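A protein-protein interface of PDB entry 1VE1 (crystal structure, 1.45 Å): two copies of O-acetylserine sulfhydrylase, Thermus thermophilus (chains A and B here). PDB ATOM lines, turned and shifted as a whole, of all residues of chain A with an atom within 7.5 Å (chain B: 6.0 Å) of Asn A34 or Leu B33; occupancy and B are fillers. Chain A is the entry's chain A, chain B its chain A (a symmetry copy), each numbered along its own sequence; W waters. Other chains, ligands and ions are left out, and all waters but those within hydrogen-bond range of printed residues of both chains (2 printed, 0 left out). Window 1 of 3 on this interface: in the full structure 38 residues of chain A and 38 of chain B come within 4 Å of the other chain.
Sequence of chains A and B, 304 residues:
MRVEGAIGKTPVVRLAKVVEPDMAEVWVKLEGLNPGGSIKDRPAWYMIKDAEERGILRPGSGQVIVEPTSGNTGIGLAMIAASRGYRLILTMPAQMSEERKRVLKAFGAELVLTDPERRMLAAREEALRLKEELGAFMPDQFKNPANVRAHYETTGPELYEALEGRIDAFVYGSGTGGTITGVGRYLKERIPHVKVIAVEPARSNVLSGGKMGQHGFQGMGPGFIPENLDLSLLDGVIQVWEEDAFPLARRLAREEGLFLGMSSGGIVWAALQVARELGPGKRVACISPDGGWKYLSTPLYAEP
Ala A6 touches Pro B11.
Pro A11 touches Ala B6.
CD2 of Leu A33 touches O of Leu B33, at 3.4 Å.
CD2 of Leu A33 touches O of Asn B34, at 3.7 Å.
Leu A33 touches Pro B35.
Asn A34 touches Leu B33 (O to CD2, 3.7 Å).
Pro A35 touches Leu B33 (CA to CD2, 3.7 Å).
O of Gly A36 touches CH2 of Trp B293 (3.3 Å).
Gly A37 touches Trp B293.
The side-chain amide nitrogen (ND2) of Asn A34 is in hydrogen-bond range of the backbone carbonyl oxygen (O) of Ser A38, 3.3 Å away.
O of Pro A11 sits at hydrogen-bond distance from N of Leu A30 (2.9 Å).
OD2 of Asp A41 is in hydrogen-bond range of N of Gly A36.
The backbone carbonyl oxygen (O) of Glu A31 sits at hydrogen-bond distance from the side-chain amide nitrogen (ND2) of Asn A34, 2.9 Å away.
The side-chain amide nitrogen (ND2) of Asn B34 lies within hydrogen-bond range of the backbone carbonyl oxygen (O) of Glu B31.
ND2 of Asn B34 lies within hydrogen-bond range of O of Ser B38, 3.3 Å away.
Of chain B, only Leu B33 (3.7 Å) comes within 4 Å of Asn A34.
Of chain A, only Leu A33 (3.4 Å), Asn A34 (3.7 Å) and Pro A35 (3.7 Å) come within 4 Å of Leu B33.
No residue of chain A comes within 4 Å of Gly B32.
Printed residues of chain B within 4 Å of Leu A33: Leu B33 (3.4 Å), Asn B34 (3.7 Å) and Pro B35 (3.7 Å).
Printed residues of chain A within 4 Å of Asn B34: Leu A33 (3.7 Å).
Of the printed residues of chain B, Pro A11 touches Ala B6 (3.8 Å).
Of the printed residues of chain B, Pro A35 touches Leu B33 (3.7 Å).
Arg A42 touches none of the printed residues of chain B.
Asp A41 touches none of the printed residues of chain B.
The nearest residue of chain B that does not touch Asn A34 is Trp B293 (5.7 Å).
The nearest residue of chain A that does not touch Leu B33 is Ala A6 (4.8 Å).
Water W1 lies within hydrogen-bond range of O of Pro A35 (2.6 Å) and NE1 of Trp B293 (3.1 Å).
Water W2 bridges O of Asn A34 (3.0 Å) and NE1 of Trp B293 (3.2 Å).
Of the 24 printed residues of chain A, 7 touch a printed residue of chain B.
Hydrophobic or aromatic side chains of chain A within 4 Å of the printed part of chain B: Ala A6, Pro A11 and Leu A33.
Of the 12 printed residues of chain B, 6 touch a printed residue of chain A.
Ala A6 touches Pro B11, and with the chains exchanged Pro A11 touches Ala B6.
Leu A33 touches its own counterpart, Leu B33.
Leu A33 touches Asn B34, and with the chains exchanged Asn A34 touches Leu B33.
Leu A33 touches Pro B35, and with the chains exchanged Pro A35 touches Leu B33.
Positions printed for both chains: 6, 10, 11, 30, 31, 32, 33, 34, 35, 37 and 38.
Of the 9 pairs that touch across the chains among the printed residues, 7 have their exchanged pair printed and touching as well.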
ATOM      1  N   VAL A   3       8.234 -11.445   2.962  1.00  0.00           N
ATOM      2  CA  VAL A   3       9.666 -11.459   3.231  1.00  0.00           C
ATOM      3  C   VAL A   3      10.342 -12.812   3.046  1.00  0.00           C
ATOM      4  O   VAL A   3      11.458 -12.878   2.534  1.00  0.00           O
ATOM      5  CB  VAL A   3       9.976 -10.903   4.642  1.00  0.00           C
ATOM      6  CG1 VAL A   3       9.548 -11.891   5.712  1.00  0.00           C
ATOM      7  CG2 VAL A   3      11.462 -10.572   4.750  1.00  0.00           C
ATOM      8  N   ALA A   6      11.764 -13.477  -0.219  1.00  0.00           N
ATOM      9  CA  ALA A   6      12.956 -12.720  -0.600  1.00  0.00           C
ATOM     10  C   ALA A   6      14.242 -13.374  -0.110  1.00  0.00           C
ATOM     11  O   ALA A   6      15.325 -12.795  -0.224  1.00  0.00           O
ATOM     12  CB  ALA A   6      12.863 -11.302  -0.055  1.00  0.00           C
ATOM     13  N   ILE A   7      14.119 -14.578   0.442  1.00  0.00           N
ATOM     14  CA  ILE A   7      15.275 -15.308   0.949  1.00  0.00           C
ATOM     15  C   ILE A   7      16.001 -16.033  -0.179  1.00  0.00           C
ATOM     16  O   ILE A   7      15.372 -16.631  -1.047  1.00  0.00           O
ATOM     17  CB  ILE A   7      14.846 -16.353   2.010  1.00  0.00           C
ATOM     18  CG1 ILE A   7      14.331 -15.642   3.264  1.00  0.00           C
ATOM     19  CG2 ILE A   7      16.015 -17.275   2.346  1.00  0.00           C
ATOM     20  CD1 ILE A   7      13.720 -16.581   4.293  1.00  0.00           C
ATOM     21  N   GLY A   8      17.328 -15.958  -0.173  1.00  0.00           N
ATOM     22  CA  GLY A   8      18.108 -16.652  -1.183  1.00  0.00           C
ATOM     23  C   GLY A   8      18.454 -15.894  -2.448  1.00  0.00           C
ATOM     24  O   GLY A   8      18.305 -14.674  -2.526  1.00  0.00           O
ATOM     25  N   LYS A   9      18.920 -16.640  -3.446  1.00  0.00           N
ATOM     26  CA  LYS A   9      19.317 -16.072  -4.731  1.00  0.00           C
ATOM     27  C   LYS A   9      20.356 -14.984  -4.497  1.00  0.00           C
ATOM     28  O   LYS A   9      20.306 -13.913  -5.099  1.00  0.00           O
ATOM     29  CB  LYS A   9      18.099 -15.494  -5.456  1.00  0.00           C
ATOM     30  CG  LYS A   9      17.034 -16.524  -5.787  1.00  0.00           C
ATOM     31  CD  LYS A   9      17.576 -17.602  -6.713  1.00  0.00           C
ATOM     32  CE  LYS A   9      16.500 -18.605  -7.091  1.00  0.00           C
ATOM     33  NZ  LYS A   9      17.027 -19.648  -8.013  1.00  0.00           N
ATOM     34  N   THR A  10      21.300 -15.281  -3.613  1.00  0.00           N
ATOM     35  CA  THR A  10      22.360 -14.352  -3.257  1.00  0.00           C
ATOM     36  C   THR A  10      23.482 -14.383  -4.286  1.00  0.00           C
ATOM     37  O   THR A  10      23.713 -15.400  -4.940  1.00  0.00           O
ATOM     38  CB  THR A  10      22.926 -14.705  -1.880  1.00  0.00           C
ATOM     39  OG1 THR A  10      23.372 -16.067  -1.894  1.00  0.00           O
ATOM     40  CG2 THR A  10      21.849 -14.533  -0.810  1.00  0.00           C
ATOM     41  N   PRO A  11      24.213 -13.268  -4.424  1.00  0.00           N
ATOM     42  CA  PRO A  11      25.312 -13.180  -5.390  1.00  0.00           C
ATOM     43  C   PRO A  11      26.618 -13.814  -4.928  1.00  0.00           C
ATOM     44  O   PRO A  11      26.824 -14.064  -3.739  1.00  0.00           O
ATOM     45  CB  PRO A  11      25.449 -11.679  -5.599  1.00  0.00           C
ATOM     46  CG  PRO A  11      25.205 -11.156  -4.219  1.00  0.00           C
ATOM     47  CD  PRO A  11      24.010 -11.976  -3.741  1.00  0.00           C
ATOM     48  N   LEU A  30      27.626 -14.284  -0.914  1.00  0.00           N
ATOM     49  CA  LEU A  30      27.246 -13.336   0.133  1.00  0.00           C
ATOM     50  C   LEU A  30      25.873 -13.555   0.753  1.00  0.00           C
ATOM     51  O   LEU A  30      24.880 -12.966   0.324  1.00  0.00           O
ATOM     52  CB  LEU A  30      27.339 -11.913  -0.429  1.00  0.00           C
ATOM     53  CG  LEU A  30      28.657 -11.591  -1.151  1.00  0.00           C
ATOM     54  CD1 LEU A  30      28.608 -10.177  -1.709  1.00  0.00           C
ATOM     55  CD2 LEU A  30      29.821 -11.750  -0.186  1.00  0.00           C
ATOM     56  N   GLU A  31      25.825 -14.382   1.790  1.00  0.00           N
ATOM     57  CA  GLU A  31      24.563 -14.686   2.456  1.00  0.00           C
ATOM     58  C   GLU A  31      24.077 -13.590   3.394  1.00  0.00           C
ATOM     59  O   GLU A  31      22.977 -13.673   3.941  1.00  0.00           O
ATOM     60  CB  GLU A  31      24.683 -16.018   3.199  1.00  0.00           C
ATOM     61  CG  GLU A  31      24.800 -17.211   2.256  1.00  0.00           C
ATOM     62  CD  GLU A  31      23.532 -17.439   1.454  1.00  0.00           C
ATOM     63  OE1 GLU A  31      23.610 -17.566   0.209  1.00  0.00           O
ATOM     64  OE2 GLU A  31      22.452 -17.498   2.072  1.00  0.00           O
ATOM     65  N   GLY A  32      24.887 -12.559   3.579  1.00  0.00           N
ATOM     66  CA  GLY A  32      24.473 -11.461   4.428  1.00  0.00           C
ATOM     67  C   GLY A  32      23.437 -10.597   3.728  1.00  0.00           C
ATOM     68  O   GLY A  32      22.821  -9.733   4.353  1.00  0.00           O
ATOM     69  N   LEU A  33      23.232 -10.828   2.433  1.00  0.00           N
ATOM     70  CA  LEU A  33      22.265 -10.039   1.675  1.00  0.00           C
ATOM     71  C   LEU A  33      20.823 -10.539   1.789  1.00  0.00           C
ATOM     72  O   LEU A  33      19.917 -10.044   1.113  1.00  0.00           O
ATOM     73  CB  LEU A  33      22.705  -9.952   0.207  1.00  0.00           C
ATOM     74  CG  LEU A  33      24.084  -9.296   0.045  1.00  0.00           C
ATOM     75  CD1 LEU A  33      24.414  -9.154  -1.428  1.00  0.00           C
ATOM     76  CD2 LEU A  33      24.101  -7.926   0.725  1.00  0.00           C
ATOM     77  N   ASN A  34      20.608 -11.513   2.664  1.00  0.00           N
ATOM     78  CA  ASN A  34      19.273 -12.047   2.900  1.00  0.00           C
ATOM     79  C   ASN A  34      18.509 -11.061   3.787  1.00  0.00           C
ATOM     80  O   ASN A  34      19.114 -10.281   4.521  1.00  0.00           O
ATOM     81  CB  ASN A  34      19.374 -13.417   3.575  1.00  0.00           C
ATOM     82  CG  ASN A  34      19.702 -14.520   2.591  1.00  0.00           C
ATOM     83  OD1 ASN A  34      18.950 -14.761   1.649  1.00  0.00           O
ATOM     84  ND2 ASN A  34      20.825 -15.193   2.799  1.00  0.00           N
ATOM     85  N   PRO A  35      17.166 -11.089   3.746  1.00  0.00           N
ATOM     86  CA  PRO A  35      16.374 -10.162   4.564  1.00  0.00           C
ATOM     87  C   PRO A  35      16.604 -10.210   6.073  1.00  0.00           C
ATOM     88  O   PRO A  35      16.395  -9.216   6.770  1.00  0.00           O
ATOM     89  CB  PRO A  35      14.933 -10.499   4.173  1.00  0.00           C
ATOM     90  CG  PRO A  35      15.010 -11.941   3.794  1.00  0.00           C
ATOM     91  CD  PRO A  35      16.291 -12.006   2.993  1.00  0.00           C
ATOM     92  N   GLY A  36      17.033 -11.362   6.578  1.00  0.00           N
ATOM     93  CA  GLY A  36      17.292 -11.499   7.996  1.00  0.00           C
ATOM     94  C   GLY A  36      18.752 -11.230   8.306  1.00  0.00           C
ATOM     95  O   GLY A  36      19.182 -11.332   9.454  1.00  0.00           O
ATOM     96  N   GLY A  37      19.517 -10.911   7.266  1.00  0.00           N
ATOM     97  CA  GLY A  37      20.925 -10.595   7.440  1.00  0.00           C
ATOM     98  C   GLY A  37      21.929 -11.732   7.430  1.00  0.00           C
ATOM     99  O   GLY A  37      23.125 -11.484   7.598  1.00  0.00           O
ATOM    100  N   SER A  38      21.479 -12.970   7.239  1.00  0.00           N
ATOM    101  CA  SER A  38      22.416 -14.088   7.231  1.00  0.00           C
ATOM    102  C   SER A  38      21.897 -15.319   6.519  1.00  0.00           C
ATOM    103  O   SER A  38      20.727 -15.404   6.138  1.00  0.00           O
ATOM    104  CB  SER A  38      22.779 -14.495   8.660  1.00  0.00           C
ATOM    105  OG  SER A  38      21.796 -15.382   9.183  1.00  0.00           O
ATOM    106  N   ILE A  39      22.797 -16.281   6.369  1.00  0.00           N
ATOM    107  CA  ILE A  39      22.504 -17.556   5.741  1.00  0.00           C
ATOM    108  C   ILE A  39      21.425 -18.315   6.519  1.00  0.00           C
ATOM    109  O   ILE A  39      20.727 -19.154   5.952  1.00  0.00           O
ATOM    110  CB  ILE A  39      23.797 -18.407   5.669  1.00  0.00           C
ATOM    111  CG1 ILE A  39      23.566 -19.665   4.837  1.00  0.00           C
ATOM    112  CG2 ILE A  39      24.273 -18.761   7.081  1.00  0.00           C
ATOM    113  CD1 ILE A  39      24.842 -20.437   4.559  1.00  0.00           C
ATOM    114  N   LYS A  40      21.280 -18.012   7.807  1.00  0.00           N
ATOM    115  CA  LYS A  40      20.292 -18.710   8.629  1.00  0.00           C
ATOM    116  C   LYS A  40      18.849 -18.481   8.213  1.00  0.00           C
ATOM    117  O   LYS A  40      17.952 -19.189   8.672  1.00  0.00           O
ATOM    118  CB  LYS A  40      20.453 -18.339  10.099  1.00  0.00           C
ATOM    119  CG  LYS A  40      21.715 -18.857  10.739  1.00  0.00           C
ATOM    120  CD  LYS A  40      21.798 -20.377  10.705  1.00  0.00           C
ATOM    121  CE  LYS A  40      22.693 -20.876  11.836  1.00  0.00           C
ATOM    122  NZ  LYS A  40      23.854 -19.971  11.830  1.00  0.00           N
ATOM    123  N   ASP A  41      18.612 -17.482   7.370  1.00  0.00           N
ATOM    124  CA  ASP A  41      17.261 -17.233   6.878  1.00  0.00           C
ATOM    125  C   ASP A  41      16.766 -18.508   6.201  1.00  0.00           C
ATOM    126  O   ASP A  41      15.599 -18.871   6.323  1.00  0.00           O
ATOM    127  CB  ASP A  41      17.256 -16.116   5.833  1.00  0.00           C
ATOM    128  CG  ASP A  41      17.252 -14.731   6.437  1.00  0.00           C
ATOM    129  OD1 ASP A  41      17.495 -14.589   7.653  1.00  0.00           O
ATOM    130  OD2 ASP A  41      17.009 -13.778   5.666  1.00  0.00           O
ATOM    131  N   ARG A  42      17.663 -19.181   5.482  1.00  0.00           N
ATOM    132  CA  ARG A  42      17.305 -20.392   4.750  1.00  0.00           C
ATOM    133  C   ARG A  42      16.827 -21.536   5.648  1.00  0.00           C
ATOM    134  O   ARG A  42      15.718 -22.040   5.465  1.00  0.00           O
ATOM    135  CB  ARG A  42      18.478 -20.838   3.864  1.00  0.00           C
ATOM    136  CG  ARG A  42      18.918 -19.797   2.817  1.00  0.00           C
ATOM    137  CD  ARG A  42      20.107 -20.324   2.017  1.00  0.00           C
ATOM    138  NE  ARG A  42      20.707 -19.346   1.104  1.00  0.00           N
ATOM    139  CZ  ARG A  42      20.425 -19.241  -0.192  1.00  0.00           C
ATOM    140  NH1 ARG A  42      19.535 -20.049  -0.755  1.00  0.00           N
ATOM    141  NH2 ARG A  42      21.067 -18.343  -0.938  1.00  0.00           N
ATOM    142  N   MET A  79      12.108 -13.346  12.255  1.00  0.00           N
ATOM    143  CA  MET A  79      11.605 -12.719  11.044  1.00  0.00           C
ATOM    144  C   MET A  79      10.460 -13.545  10.465  1.00  0.00           C
ATOM    145  O   MET A  79       9.400 -13.007  10.136  1.00  0.00           O
ATOM    146  CB  MET A  79      12.731 -12.598  10.021  1.00  0.00           C
ATOM    147  CG  MET A  79      12.289 -12.040   8.681  1.00  0.00           C
ATOM    148  SD  MET A  79      13.671 -11.937   7.529  1.00  0.00           S
ATOM    149  CE  MET A  79      13.838 -13.661   7.064  1.00  0.00           C
ATOM    150  N   GLU A 158      22.216 -22.917  -6.302  1.00  0.00           N
ATOM    151  CA  GLU A 158      22.604 -21.550  -6.638  1.00  0.00           C
ATOM    152  C   GLU A 158      24.106 -21.423  -6.859  1.00  0.00           C
ATOM    153  O   GLU A 158      24.549 -20.811  -7.835  1.00  0.00           O
ATOM    154  CB  GLU A 158      22.195 -20.585  -5.524  1.00  0.00           C
ATOM    155  CG  GLU A 158      20.709 -20.304  -5.426  1.00  0.00           C
ATOM    156  CD  GLU A 158      20.381 -19.432  -4.230  1.00  0.00           C
ATOM    157  OE1 GLU A 158      21.263 -18.656  -3.806  1.00  0.00           O
ATOM    158  OE2 GLU A 158      19.244 -19.511  -3.719  1.00  0.00           O
ATOM    159  N   SER A 288      30.049 -16.645   2.712  1.00  0.00           N
ATOM    160  CA  SER A 288      30.113 -15.658   3.784  1.00  0.00           C
ATOM    161  C   SER A 288      28.757 -15.748   4.481  1.00  0.00           C
ATOM    162  O   SER A 288      27.734 -15.382   3.913  1.00  0.00           O
ATOM    163  CB  SER A 288      30.303 -14.250   3.214  1.00  0.00           C
ATOM    164  OG  SER A 288      30.038 -13.267   4.206  1.00  0.00           O
ATOM    165  N   PRO A 289      28.733 -16.248   5.722  1.00  0.00           N
ATOM    166  CA  PRO A 289      27.467 -16.376   6.453  1.00  0.00           C
ATOM    167  C   PRO A 289      26.699 -15.076   6.684  1.00  0.00           C
ATOM    168  O   PRO A 289      25.469 -15.062   6.631  1.00  0.00           O
ATOM    169  CB  PRO A 289      27.895 -17.040   7.751  1.00  0.00           C
ATOM    170  CG  PRO A 289      29.076 -17.870   7.324  1.00  0.00           C
ATOM    171  CD  PRO A 289      29.829 -16.908   6.448  1.00  0.00           C
ATOM    172  N   ALA B   6      27.050  -6.702  -7.595  1.00  0.00           N
ATOM    173  CA  ALA B   6      25.994  -7.261  -6.754  1.00  0.00           C
ATOM    174  C   ALA B   6      24.978  -6.211  -6.320  1.00  0.00           C
ATOM    175  O   ALA B   6      24.103  -6.487  -5.495  1.00  0.00           O
ATOM    176  CB  ALA B   6      26.606  -7.920  -5.526  1.00  0.00           C
ATOM    177  N   THR B  10      16.880  -5.825  -6.368  1.00  0.00           N
ATOM    178  CA  THR B  10      16.311  -6.036  -5.047  1.00  0.00           C
ATOM    179  C   THR B  10      14.860  -6.488  -5.143  1.00  0.00           C
ATOM    180  O   THR B  10      14.158  -6.158  -6.099  1.00  0.00           O
ATOM    181  CB  THR B  10      16.388  -4.744  -4.231  1.00  0.00           C
ATOM    182  OG1 THR B  10      15.725  -3.698  -4.952  1.00  0.00           O
ATOM    183  CG2 THR B  10      17.847  -4.357  -3.996  1.00  0.00           C
ATOM    184  N   PRO B  11      14.385  -7.228  -4.133  1.00  0.00           N
ATOM    185  CA  PRO B  11      13.005  -7.725  -4.122  1.00  0.00           C
ATOM    186  C   PRO B  11      11.964  -6.705  -3.681  1.00  0.00           C
ATOM    187  O   PRO B  11      12.284  -5.684  -3.071  1.00  0.00           O
ATOM    188  CB  PRO B  11      13.086  -8.907  -3.167  1.00  0.00           C
ATOM    189  CG  PRO B  11      14.038  -8.396  -2.132  1.00  0.00           C
ATOM    190  CD  PRO B  11      15.130  -7.727  -2.960  1.00  0.00           C
ATOM    191  N   LEU B  30      12.851  -3.463  -1.222  1.00  0.00           N
ATOM    192  CA  LEU B  30      13.850  -3.506  -0.155  1.00  0.00           C
ATOM    193  C   LEU B  30      15.281  -3.203  -0.579  1.00  0.00           C
ATOM    194  O   LEU B  30      16.058  -4.106  -0.887  1.00  0.00           O
ATOM    195  CB  LEU B  30      13.791  -4.878   0.525  1.00  0.00           C
ATOM    196  CG  LEU B  30      12.382  -5.334   0.935  1.00  0.00           C
ATOM    197  CD1 LEU B  30      12.446  -6.725   1.545  1.00  0.00           C
ATOM    198  CD2 LEU B  30      11.790  -4.339   1.920  1.00  0.00           C
ATOM    199  N   GLU B  31      15.637  -1.923  -0.562  1.00  0.00           N
ATOM    200  CA  GLU B  31      16.975  -1.508  -0.965  1.00  0.00           C
ATOM    201  C   GLU B  31      18.045  -1.751   0.089  1.00  0.00           C
ATOM    202  O   GLU B  31      19.232  -1.540  -0.158  1.00  0.00           O
ATOM    203  CB  GLU B  31      16.952  -0.036  -1.382  1.00  0.00           C
ATOM    204  CG  GLU B  31      16.180   0.199  -2.676  1.00  0.00           C
ATOM    205  CD  GLU B  31      16.861  -0.431  -3.876  1.00  0.00           C
ATOM    206  OE1 GLU B  31      16.194  -1.165  -4.642  1.00  0.00           O
ATOM    207  OE2 GLU B  31      18.069  -0.185  -4.059  1.00  0.00           O
ATOM    208  N   GLY B  32      17.633  -2.199   1.266  1.00  0.00           N
ATOM    209  CA  GLY B  32      18.601  -2.488   2.304  1.00  0.00           C
ATOM    210  C   GLY B  32      19.345  -3.779   2.008  1.00  0.00           C
ATOM    211  O   GLY B  32      20.337  -4.094   2.665  1.00  0.00           O
ATOM    212  N   LEU B  33      18.878  -4.530   1.011  1.00  0.00           N
ATOM    213  CA  LEU B  33      19.521  -5.794   0.660  1.00  0.00           C
ATOM    214  C   LEU B  33      20.723  -5.646  -0.277  1.00  0.00           C
ATOM    215  O   LEU B  33      21.292  -6.633  -0.750  1.00  0.00           O
ATOM    216  CB  LEU B  33      18.481  -6.759   0.077  1.00  0.00           C
ATOM    217  CG  LEU B  33      17.343  -7.062   1.063  1.00  0.00           C
ATOM    218  CD1 LEU B  33      16.405  -8.092   0.462  1.00  0.00           C
ATOM    219  CD2 LEU B  33      17.912  -7.573   2.385  1.00  0.00           C
ATOM    220  N   ASN B  34      21.119  -4.405  -0.529  1.00  0.00           N
ATOM    221  CA  ASN B  34      22.278  -4.130  -1.370  1.00  0.00           C
ATOM    222  C   ASN B  34      23.542  -4.383  -0.546  1.00  0.00           C
ATOM    223  O   ASN B  34      23.511  -4.323   0.683  1.00  0.00           O
ATOM    224  CB  ASN B  34      22.231  -2.681  -1.859  1.00  0.00           C
ATOM    225  CG  ASN B  34      21.275  -2.495  -3.019  1.00  0.00           C
ATOM    226  OD1 ASN B  34      21.443  -3.108  -4.072  1.00  0.00           O
ATOM    227  ND2 ASN B  34      20.267  -1.655  -2.835  1.00  0.00           N
ATOM    228  N   PRO B  35      24.679  -4.657  -1.209  1.00  0.00           N
ATOM    229  CA  PRO B  35      25.925  -4.920  -0.477  1.00  0.00           C
ATOM    230  C   PRO B  35      26.413  -3.822   0.466  1.00  0.00           C
ATOM    231  O   PRO B  35      27.111  -4.100   1.441  1.00  0.00           O
ATOM    232  CB  PRO B  35      26.924  -5.229  -1.595  1.00  0.00           C
ATOM    233  CG  PRO B  35      26.398  -4.445  -2.750  1.00  0.00           C
ATOM    234  CD  PRO B  35      24.908  -4.685  -2.664  1.00  0.00           C
ATOM    235  N   GLY B  37      24.305  -1.944   2.024  1.00  0.00           N
ATOM    236  CA  GLY B  37      23.230  -1.773   2.987  1.00  0.00           C
ATOM    237  C   GLY B  37      22.133  -0.773   2.677  1.00  0.00           C
ATOM    238  O   GLY B  37      21.225  -0.599   3.494  1.00  0.00           O
ATOM    239  N   SER B  38      22.189  -0.110   1.524  1.00  0.00           N
ATOM    240  CA  SER B  38      21.154   0.864   1.197  1.00  0.00           C
ATOM    241  C   SER B  38      21.031   1.157  -0.284  1.00  0.00           C
ATOM    242  O   SER B  38      21.850   0.730  -1.099  1.00  0.00           O
ATOM    243  CB  SER B  38      21.419   2.191   1.913  1.00  0.00           C
ATOM    244  OG  SER B  38      22.334   2.980   1.162  1.00  0.00           O
ATOM    245  N   TRP B 293      19.340  -2.325  10.564  1.00  0.00           N
ATOM    246  CA  TRP B 293      20.654  -2.681  11.104  1.00  0.00           C
ATOM    247  C   TRP B 293      21.539  -1.573  11.658  1.00  0.00           C
ATOM    248  O   TRP B 293      22.234  -1.781  12.654  1.00  0.00           O
ATOM    249  CB  TRP B 293      21.444  -3.473  10.058  1.00  0.00           C
ATOM    250  CG  TRP B 293      20.673  -4.637   9.526  1.00  0.00           C
ATOM    251  CD1 TRP B 293      20.019  -4.708   8.336  1.00  0.00           C
ATOM    252  CD2 TRP B 293      20.396  -5.865  10.211  1.00  0.00           C
ATOM    253  NE1 TRP B 293      19.342  -5.900   8.231  1.00  0.00           N
ATOM    254  CE2 TRP B 293      19.558  -6.631   9.371  1.00  0.00           C
ATOM    255  CE3 TRP B 293      20.772  -6.390  11.455  1.00  0.00           C
ATOM    256  CZ2 TRP B 293      19.086  -7.896   9.733  1.00  0.00           C
ATOM    257  CZ3 TRP B 293      20.302  -7.650  11.815  1.00  0.00           C
ATOM    258  CH2 TRP B 293      19.467  -8.387  10.956  1.00  0.00           C
HETATM  259  O   HOH W   1      17.177  -6.845   6.201  1.00  0.00           O
HETATM  260  O   HOH W   2      19.791  -7.555   5.545  1.00  0.00           O
